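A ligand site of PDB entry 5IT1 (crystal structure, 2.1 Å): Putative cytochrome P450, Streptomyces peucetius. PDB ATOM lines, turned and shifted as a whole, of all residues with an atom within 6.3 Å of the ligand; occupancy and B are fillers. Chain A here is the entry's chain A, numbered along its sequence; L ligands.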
ATOM      1  N   LYS A  81      -7.683  -5.964 -21.815  1.00  0.00           N
ATOM      2  CA  LYS A  81      -8.924  -6.230 -22.577  1.00  0.00           C
ATOM      3  C   LYS A  81      -9.704  -4.957 -22.818  1.00  0.00           C
ATOM      4  O   LYS A  81      -9.641  -4.034 -22.017  1.00  0.00           O
ATOM      5  CB  LYS A  81      -9.828  -7.127 -21.723  1.00  0.00           C
ATOM      6  CG  LYS A  81      -9.248  -8.490 -21.387  1.00  0.00           C
ATOM      7  CD  LYS A  81      -9.037  -9.314 -22.625  1.00  0.00           C
ATOM      8  CE  LYS A  81      -8.430 -10.692 -22.331  1.00  0.00           C
ATOM      9  NZ  LYS A  81      -6.970 -10.749 -22.709  1.00  0.00           N
ATOM     10  N   PRO A  82     -10.557  -4.929 -23.840  1.00  0.00           N
ATOM     11  CA  PRO A  82     -11.448  -3.798 -24.018  1.00  0.00           C
ATOM     12  C   PRO A  82     -12.473  -3.692 -22.941  1.00  0.00           C
ATOM     13  O   PRO A  82     -12.682  -4.669 -22.190  1.00  0.00           O
ATOM     14  CB  PRO A  82     -12.168  -4.137 -25.285  1.00  0.00           C
ATOM     15  CG  PRO A  82     -11.298  -4.994 -26.003  1.00  0.00           C
ATOM     16  CD  PRO A  82     -10.578  -5.826 -24.994  1.00  0.00           C
ATOM     17  N   GLY A  83     -13.171  -2.564 -22.914  1.00  0.00           N
ATOM     18  CA  GLY A  83     -14.099  -2.257 -21.830  1.00  0.00           C
ATOM     19  C   GLY A  83     -15.565  -2.502 -22.241  1.00  0.00           C
ATOM     20  O   GLY A  83     -15.863  -3.339 -23.055  1.00  0.00           O
ATOM     21  N   SER A  86     -17.783  -4.747 -24.975  1.00  0.00           N
ATOM     22  CA  SER A  86     -17.084  -5.892 -25.564  1.00  0.00           C
ATOM     23  C   SER A  86     -17.530  -7.290 -25.146  1.00  0.00           C
ATOM     24  O   SER A  86     -17.288  -8.220 -25.919  1.00  0.00           O
ATOM     25  CB  SER A  86     -15.540  -5.772 -25.486  1.00  0.00           C
ATOM     26  OG  SER A  86     -15.117  -5.760 -24.147  1.00  0.00           O
ATOM     27  N   LEU A  88     -16.995 -10.111 -23.766  1.00  0.00           N
ATOM     28  CA  LEU A  88     -16.380 -11.428 -23.567  1.00  0.00           C
ATOM     29  C   LEU A  88     -15.721 -11.565 -22.219  1.00  0.00           C
ATOM     30  O   LEU A  88     -15.680 -12.658 -21.698  1.00  0.00           O
ATOM     31  CB  LEU A  88     -15.315 -11.727 -24.599  1.00  0.00           C
ATOM     32  CG  LEU A  88     -15.745 -12.447 -25.872  1.00  0.00           C
ATOM     33  CD1 LEU A  88     -16.418 -11.441 -26.781  1.00  0.00           C
ATOM     34  CD2 LEU A  88     -14.540 -12.936 -26.661  1.00  0.00           C
ATOM     35  N   TRP A  89     -15.253 -10.470 -21.645  1.00  0.00           N
ATOM     36  CA  TRP A  89     -14.490 -10.460 -20.422  1.00  0.00           C
ATOM     37  C   TRP A  89     -15.210  -9.704 -19.360  1.00  0.00           C
ATOM     38  O   TRP A  89     -14.610  -9.370 -18.365  1.00  0.00           O
ATOM     39  CB  TRP A  89     -13.117  -9.841 -20.705  1.00  0.00           C
ATOM     40  CG  TRP A  89     -12.415 -10.641 -21.761  1.00  0.00           C
ATOM     41  CD1 TRP A  89     -11.909 -11.913 -21.640  1.00  0.00           C
ATOM     42  CD2 TRP A  89     -12.277 -10.293 -23.135  1.00  0.00           C
ATOM     43  NE1 TRP A  89     -11.413 -12.336 -22.842  1.00  0.00           N
ATOM     44  CE2 TRP A  89     -11.627 -11.358 -23.784  1.00  0.00           C
ATOM     45  CE3 TRP A  89     -12.634  -9.167 -23.879  1.00  0.00           C
ATOM     46  CZ2 TRP A  89     -11.349 -11.351 -25.152  1.00  0.00           C
ATOM     47  CZ3 TRP A  89     -12.336  -9.153 -25.236  1.00  0.00           C
ATOM     48  CH2 TRP A  89     -11.692 -10.240 -25.860  1.00  0.00           C
ATOM     49  N   MET A 172      -7.093  -8.441 -38.822  1.00  0.00           N
ATOM     50  CA  MET A 172      -7.507  -8.778 -37.488  1.00  0.00           C
ATOM     51  C   MET A 172      -7.760 -10.251 -37.264  1.00  0.00           C
ATOM     52  O   MET A 172      -7.592 -10.771 -36.171  1.00  0.00           O
ATOM     53  CB  MET A 172      -8.739  -7.935 -37.060  1.00  0.00           C
ATOM     54  CG  MET A 172      -9.020  -7.891 -35.528  1.00  0.00           C
ATOM     55  SD  MET A 172      -7.800  -7.105 -34.374  1.00  0.00           S
ATOM     56  CE  MET A 172      -7.198  -6.128 -35.693  1.00  0.00           C
ATOM     57  N   GLN A 177      -8.477 -13.037 -30.509  1.00  0.00           N
ATOM     58  CA  GLN A 177      -9.434 -12.108 -29.936  1.00  0.00           C
ATOM     59  C   GLN A 177      -8.865 -11.559 -28.619  1.00  0.00           C
ATOM     60  O   GLN A 177      -8.987 -10.352 -28.365  1.00  0.00           O
ATOM     61  CB  GLN A 177     -10.833 -12.740 -29.699  1.00  0.00           C
ATOM     62  CG  GLN A 177     -11.828 -11.712 -29.178  1.00  0.00           C
ATOM     63  CD  GLN A 177     -13.266 -11.741 -29.851  1.00  0.00           C
ATOM     64  OE1 GLN A 177     -13.730 -12.770 -30.377  1.00  0.00           O
ATOM     65  NE2 GLN A 177     -13.970 -10.587 -29.781  1.00  0.00           N
ATOM     66  N   ALA A 180      -6.319  -8.659 -29.190  1.00  0.00           N
ATOM     67  CA  ALA A 180      -6.710  -7.582 -30.179  1.00  0.00           C
ATOM     68  C   ALA A 180      -6.447  -6.170 -29.655  1.00  0.00           C
ATOM     69  O   ALA A 180      -5.878  -5.267 -30.348  1.00  0.00           O
ATOM     70  CB  ALA A 180      -8.205  -7.722 -30.554  1.00  0.00           C
ATOM     71  N   ALA A 181      -6.884  -5.999 -28.423  1.00  0.00           N
ATOM     72  CA  ALA A 181      -6.811  -4.725 -27.739  1.00  0.00           C
ATOM     73  C   ALA A 181      -5.342  -4.260 -27.443  1.00  0.00           C
ATOM     74  O   ALA A 181      -5.154  -3.117 -27.023  1.00  0.00           O
ATOM     75  CB  ALA A 181      -7.649  -4.783 -26.457  1.00  0.00           C
ATOM     76  N   THR A 182      -4.335  -5.143 -27.633  1.00  0.00           N
ATOM     77  CA  THR A 182      -2.937  -4.778 -27.458  1.00  0.00           C
ATOM     78  C   THR A 182      -2.067  -5.099 -28.716  1.00  0.00           C
ATOM     79  O   THR A 182      -0.876  -5.243 -28.609  1.00  0.00           O
ATOM     80  CB  THR A 182      -2.368  -5.523 -26.233  1.00  0.00           C
ATOM     81  OG1 THR A 182      -2.613  -6.923 -26.394  1.00  0.00           O
ATOM     82  CG2 THR A 182      -3.072  -5.053 -24.900  1.00  0.00           C
ATOM     83  N   GLU A 183      -2.681  -5.230 -29.886  1.00  0.00           N
ATOM     84  CA  GLU A 183      -1.942  -5.469 -31.127  1.00  0.00           C
ATOM     85  C   GLU A 183      -2.112  -4.317 -32.099  1.00  0.00           C
ATOM     86  O   GLU A 183      -3.108  -3.608 -32.038  1.00  0.00           O
ATOM     87  CB  GLU A 183      -2.471  -6.732 -31.841  1.00  0.00           C
ATOM     88  CG  GLU A 183      -1.973  -8.024 -31.227  1.00  0.00           C
ATOM     89  CD  GLU A 183      -0.494  -8.268 -31.467  1.00  0.00           C
ATOM     90  OE1 GLU A 183      -0.017  -8.023 -32.607  1.00  0.00           O
ATOM     91  OE2 GLU A 183       0.202  -8.682 -30.499  1.00  0.00           O
ATOM     92  N   ALA A 185      -2.965  -4.422 -35.235  1.00  0.00           N
ATOM     93  CA  ALA A 185      -4.070  -4.486 -36.179  1.00  0.00           C
ATOM     94  C   ALA A 185      -5.272  -3.962 -35.452  1.00  0.00           C
ATOM     95  O   ALA A 185      -6.203  -3.426 -36.047  1.00  0.00           O
ATOM     96  CB  ALA A 185      -4.287  -5.921 -36.652  1.00  0.00           C
ATOM     97  N   GLY A 186      -5.299  -4.140 -34.129  1.00  0.00           N
ATOM     98  CA  GLY A 186      -6.361  -3.572 -33.302  1.00  0.00           C
ATOM     99  C   GLY A 186      -6.507  -2.072 -33.391  1.00  0.00           C
ATOM    100  O   GLY A 186      -7.614  -1.539 -33.369  1.00  0.00           O
ATOM    101  N   MET A 187      -5.391  -1.387 -33.530  1.00  0.00           N
ATOM    102  CA  MET A 187      -5.455   0.067 -33.616  1.00  0.00           C
ATOM    103  C   MET A 187      -6.048   0.486 -34.941  1.00  0.00           C
ATOM    104  O   MET A 187      -6.776   1.474 -35.046  1.00  0.00           O
ATOM    105  CB  MET A 187      -4.075   0.699 -33.459  1.00  0.00           C
ATOM    106  CG  MET A 187      -3.442   0.477 -32.088  1.00  0.00           C
ATOM    107  SD  MET A 187      -4.323   1.383 -30.805  1.00  0.00           S
ATOM    108  CE  MET A 187      -4.535   0.061 -29.586  1.00  0.00           C
ATOM    109  N   LEU A 189      -8.139  -1.222 -36.835  1.00  0.00           N
ATOM    110  CA  LEU A 189      -9.608  -1.465 -36.701  1.00  0.00           C
ATOM    111  C   LEU A 189     -10.304  -0.407 -35.821  1.00  0.00           C
ATOM    112  O   LEU A 189     -11.358   0.120 -36.156  1.00  0.00           O
ATOM    113  CB  LEU A 189      -9.879  -2.866 -36.151  1.00  0.00           C
ATOM    114  CG  LEU A 189     -11.370  -3.195 -35.963  1.00  0.00           C
ATOM    115  CD1 LEU A 189     -12.090  -3.055 -37.314  1.00  0.00           C
ATOM    116  CD2 LEU A 189     -11.501  -4.593 -35.428  1.00  0.00           C
ATOM    117  N   GLY A 190      -9.710  -0.064 -34.691  1.00  0.00           N
ATOM    118  CA  GLY A 190     -10.234   1.012 -33.890  1.00  0.00           C
ATOM    119  C   GLY A 190     -10.491   2.275 -34.707  1.00  0.00           C
ATOM    120  O   GLY A 190     -11.524   2.918 -34.538  1.00  0.00           O
ATOM    121  N   LEU A 193     -13.442   1.802 -37.034  1.00  0.00           N
ATOM    122  CA  LEU A 193     -14.726   1.838 -36.326  1.00  0.00           C
ATOM    123  C   LEU A 193     -15.097   3.207 -35.823  1.00  0.00           C
ATOM    124  O   LEU A 193     -16.324   3.581 -35.831  1.00  0.00           O
ATOM    125  CB  LEU A 193     -14.752   0.877 -35.176  1.00  0.00           C
ATOM    126  CG  LEU A 193     -14.649  -0.587 -35.567  1.00  0.00           C
ATOM    127  CD1 LEU A 193     -14.643  -1.394 -34.269  1.00  0.00           C
ATOM    128  CD2 LEU A 193     -15.782  -1.068 -36.496  1.00  0.00           C
ATOM    129  N   MET A 225     -17.295   4.886 -27.521  1.00  0.00           N
ATOM    130  CA  MET A 225     -16.399   3.805 -27.093  1.00  0.00           C
ATOM    131  C   MET A 225     -17.216   2.517 -26.924  1.00  0.00           C
ATOM    132  O   MET A 225     -16.806   1.449 -27.371  1.00  0.00           O
ATOM    133  CB  MET A 225     -15.707   4.245 -25.782  1.00  0.00           C
ATOM    134  CG  MET A 225     -14.425   3.488 -25.428  1.00  0.00           C
ATOM    135  SD  MET A 225     -13.107   3.484 -26.661  1.00  0.00           S
ATOM    136  CE  MET A 225     -13.427   5.114 -27.133  1.00  0.00           C
ATOM    137  N   MET A 228     -17.942   1.215 -30.364  1.00  0.00           N
ATOM    138  CA  MET A 228     -16.744   0.671 -31.045  1.00  0.00           C
ATOM    139  C   MET A 228     -16.418  -0.682 -30.458  1.00  0.00           C
ATOM    140  O   MET A 228     -16.069  -1.608 -31.166  1.00  0.00           O
ATOM    141  CB  MET A 228     -15.576   1.613 -30.920  1.00  0.00           C
ATOM    142  CG  MET A 228     -15.572   2.725 -31.961  1.00  0.00           C
ATOM    143  SD  MET A 228     -14.235   3.907 -31.614  1.00  0.00           S
ATOM    144  CE  MET A 228     -14.871   4.707 -30.217  1.00  0.00           C
ATOM    145  N   ASN A 229     -16.590  -0.803 -29.160  1.00  0.00           N
ATOM    146  CA  ASN A 229     -16.316  -2.065 -28.474  1.00  0.00           C
ATOM    147  C   ASN A 229     -17.310  -3.143 -28.883  1.00  0.00           C
ATOM    148  O   ASN A 229     -16.955  -4.285 -29.017  1.00  0.00           O
ATOM    149  CB  ASN A 229     -16.371  -1.909 -26.965  1.00  0.00           C
ATOM    150  CG  ASN A 229     -15.092  -1.289 -26.431  1.00  0.00           C
ATOM    151  OD1 ASN A 229     -14.083  -1.316 -27.071  1.00  0.00           O
ATOM    152  ND2 ASN A 229     -15.172  -0.668 -25.336  1.00  0.00           N
ATOM    153  N   ALA A 230     -18.557  -2.774 -29.086  1.00  0.00           N
ATOM    154  CA  ALA A 230     -19.569  -3.750 -29.451  1.00  0.00           C
ATOM    155  C   ALA A 230     -19.347  -4.124 -30.862  1.00  0.00           C
ATOM    156  O   ALA A 230     -19.371  -5.298 -31.162  1.00  0.00           O
ATOM    157  CB  ALA A 230     -20.985  -3.231 -29.224  1.00  0.00           C
ATOM    158  N   ALA A 231     -19.059  -3.197 -31.730  1.00  0.00           N
ATOM    159  CA  ALA A 231     -18.918  -3.560 -33.139  1.00  0.00           C
ATOM    160  C   ALA A 231     -17.693  -4.357 -33.339  1.00  0.00           C
ATOM    161  O   ALA A 231     -17.593  -5.225 -34.202  1.00  0.00           O
ATOM    162  CB  ALA A 231     -18.837  -2.371 -34.005  1.00  0.00           C
ATOM    163  N   GLY A 232     -16.657  -3.928 -32.672  1.00  0.00           N
ATOM    164  CA  GLY A 232     -15.413  -4.668 -32.774  1.00  0.00           C
ATOM    165  C   GLY A 232     -15.554  -6.073 -32.329  1.00  0.00           C
ATOM    166  O   GLY A 232     -15.054  -6.978 -32.937  1.00  0.00           O
ATOM    167  N   THR A 233     -16.246  -6.259 -31.215  1.00  0.00           N
ATOM    168  CA  THR A 233     -16.360  -7.571 -30.680  1.00  0.00           C
ATOM    169  C   THR A 233     -17.215  -8.426 -31.633  1.00  0.00           C
ATOM    170  O   THR A 233     -16.878  -9.578 -31.845  1.00  0.00           O
ATOM    171  CB  THR A 233     -16.957  -7.501 -29.275  1.00  0.00           C
ATOM    172  OG1 THR A 233     -15.982  -7.880 -28.325  1.00  0.00           O
ATOM    173  CG2 THR A 233     -18.132  -8.430 -29.089  1.00  0.00           C
ATOM    174  N   LEU A 234     -18.324  -7.886 -32.206  1.00  0.00           N
ATOM    175  CA  LEU A 234     -19.097  -8.641 -33.116  1.00  0.00           C
ATOM    176  C   LEU A 234     -18.222  -9.074 -34.258  1.00  0.00           C
ATOM    177  O   LEU A 234     -18.226 -10.223 -34.647  1.00  0.00           O
ATOM    178  CB  LEU A 234     -20.340  -7.842 -33.653  1.00  0.00           C
ATOM    179  CG  LEU A 234     -21.397  -7.620 -32.567  1.00  0.00           C
ATOM    180  CD1 LEU A 234     -22.559  -6.801 -33.105  1.00  0.00           C
ATOM    181  CD2 LEU A 234     -21.945  -8.925 -32.055  1.00  0.00           C
ATOM    182  N   ILE A 236     -14.873  -9.406 -34.718  1.00  0.00           N
ATOM    183  CA  ILE A 236     -13.812 -10.375 -34.415  1.00  0.00           C
ATOM    184  C   ILE A 236     -14.379 -11.708 -33.989  1.00  0.00           C
ATOM    185  O   ILE A 236     -13.859 -12.687 -34.423  1.00  0.00           O
ATOM    186  CB  ILE A 236     -12.884  -9.849 -33.324  1.00  0.00           C
ATOM    187  CG1 ILE A 236     -12.158  -8.605 -33.882  1.00  0.00           C
ATOM    188  CG2 ILE A 236     -11.845 -10.927 -32.966  1.00  0.00           C
ATOM    189  CD1 ILE A 236     -11.597  -7.681 -32.845  1.00  0.00           C
HETATM  190  O1  LIG L   1     -13.428  -7.739 -28.399  1.00  0.00           O
HETATM  191  C1  LIG L   1     -12.971  -6.560 -28.942  1.00  0.00           C
HETATM  192  C2  LIG L   1     -13.769  -5.439 -29.103  1.00  0.00           C
HETATM  193  C3  LIG L   1     -13.240  -4.263 -29.645  1.00  0.00           C
HETATM  194  C4  LIG L   1     -11.620  -6.451 -29.271  1.00  0.00           C
HETATM  195  C5  LIG L   1     -11.100  -5.292 -29.798  1.00  0.00           C
HETATM  196  C6  LIG L   1     -11.882  -4.174 -30.005  1.00  0.00           C
HETATM  197  C7  LIG L   1     -11.236  -2.909 -30.556  1.00  0.00           C
HETATM  198  C8  LIG L   1     -12.274  -1.808 -30.708  1.00  0.00           C
HETATM  199  C9  LIG L   1     -10.619  -3.154 -31.906  1.00  0.00           C
HETATM  200  C10 LIG L   1     -10.176  -2.337 -29.635  1.00  0.00           C
HETATM  201  C11 LIG L   1     -10.561  -2.017 -28.347  1.00  0.00           C
HETATM  202  C12 LIG L   1      -9.711  -1.455 -27.417  1.00  0.00           C
HETATM  203  C13 LIG L   1      -8.846  -2.063 -30.024  1.00  0.00           C
HETATM  204  C14 LIG L   1      -7.974  -1.499 -29.074  1.00  0.00           C
HETATM  205  C15 LIG L   1      -8.400  -1.204 -27.802  1.00  0.00           C
HETATM  206  O2  LIG L   1      -7.572  -0.676 -26.895  1.00  0.00           O
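Residues that only touch the ligand: Asn 229, Pro 82, Gly 186, Trp 89, Gly 232, Ile 236, Met 187, Met 228, Ala 180 and Leu 189.
Of the 27 residues printed, 13 come within 4 Å of the ligand.
An oxygen (O1) of the ligand is in hydrogen-bond range of the side-chain amide nitrogen (NE2) of Gln 177 (3.2 Å).
OG1 of Thr 233 is in hydrogen-bond range of O1 of the ligand (2.6 Å).
An oxygen (O2) of the ligand sits at hydrogen-bond distance from the backbone carbonyl oxygen of Ala 181, 3.4 Å away.
The side-chain hydroxyl of Thr 233 lies within hydrogen-bond range of the backbone carbonyl oxygen of Ser 86 (2.8 Å).
The backbone carbonyl oxygen of Pro 82 is in hydrogen-bond range of the side-chain hydroxyl of Ser 86 (3.3 Å).
ND2 of Asn 229 lies within hydrogen-bond range of O of Met 225 (3.4 Å).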
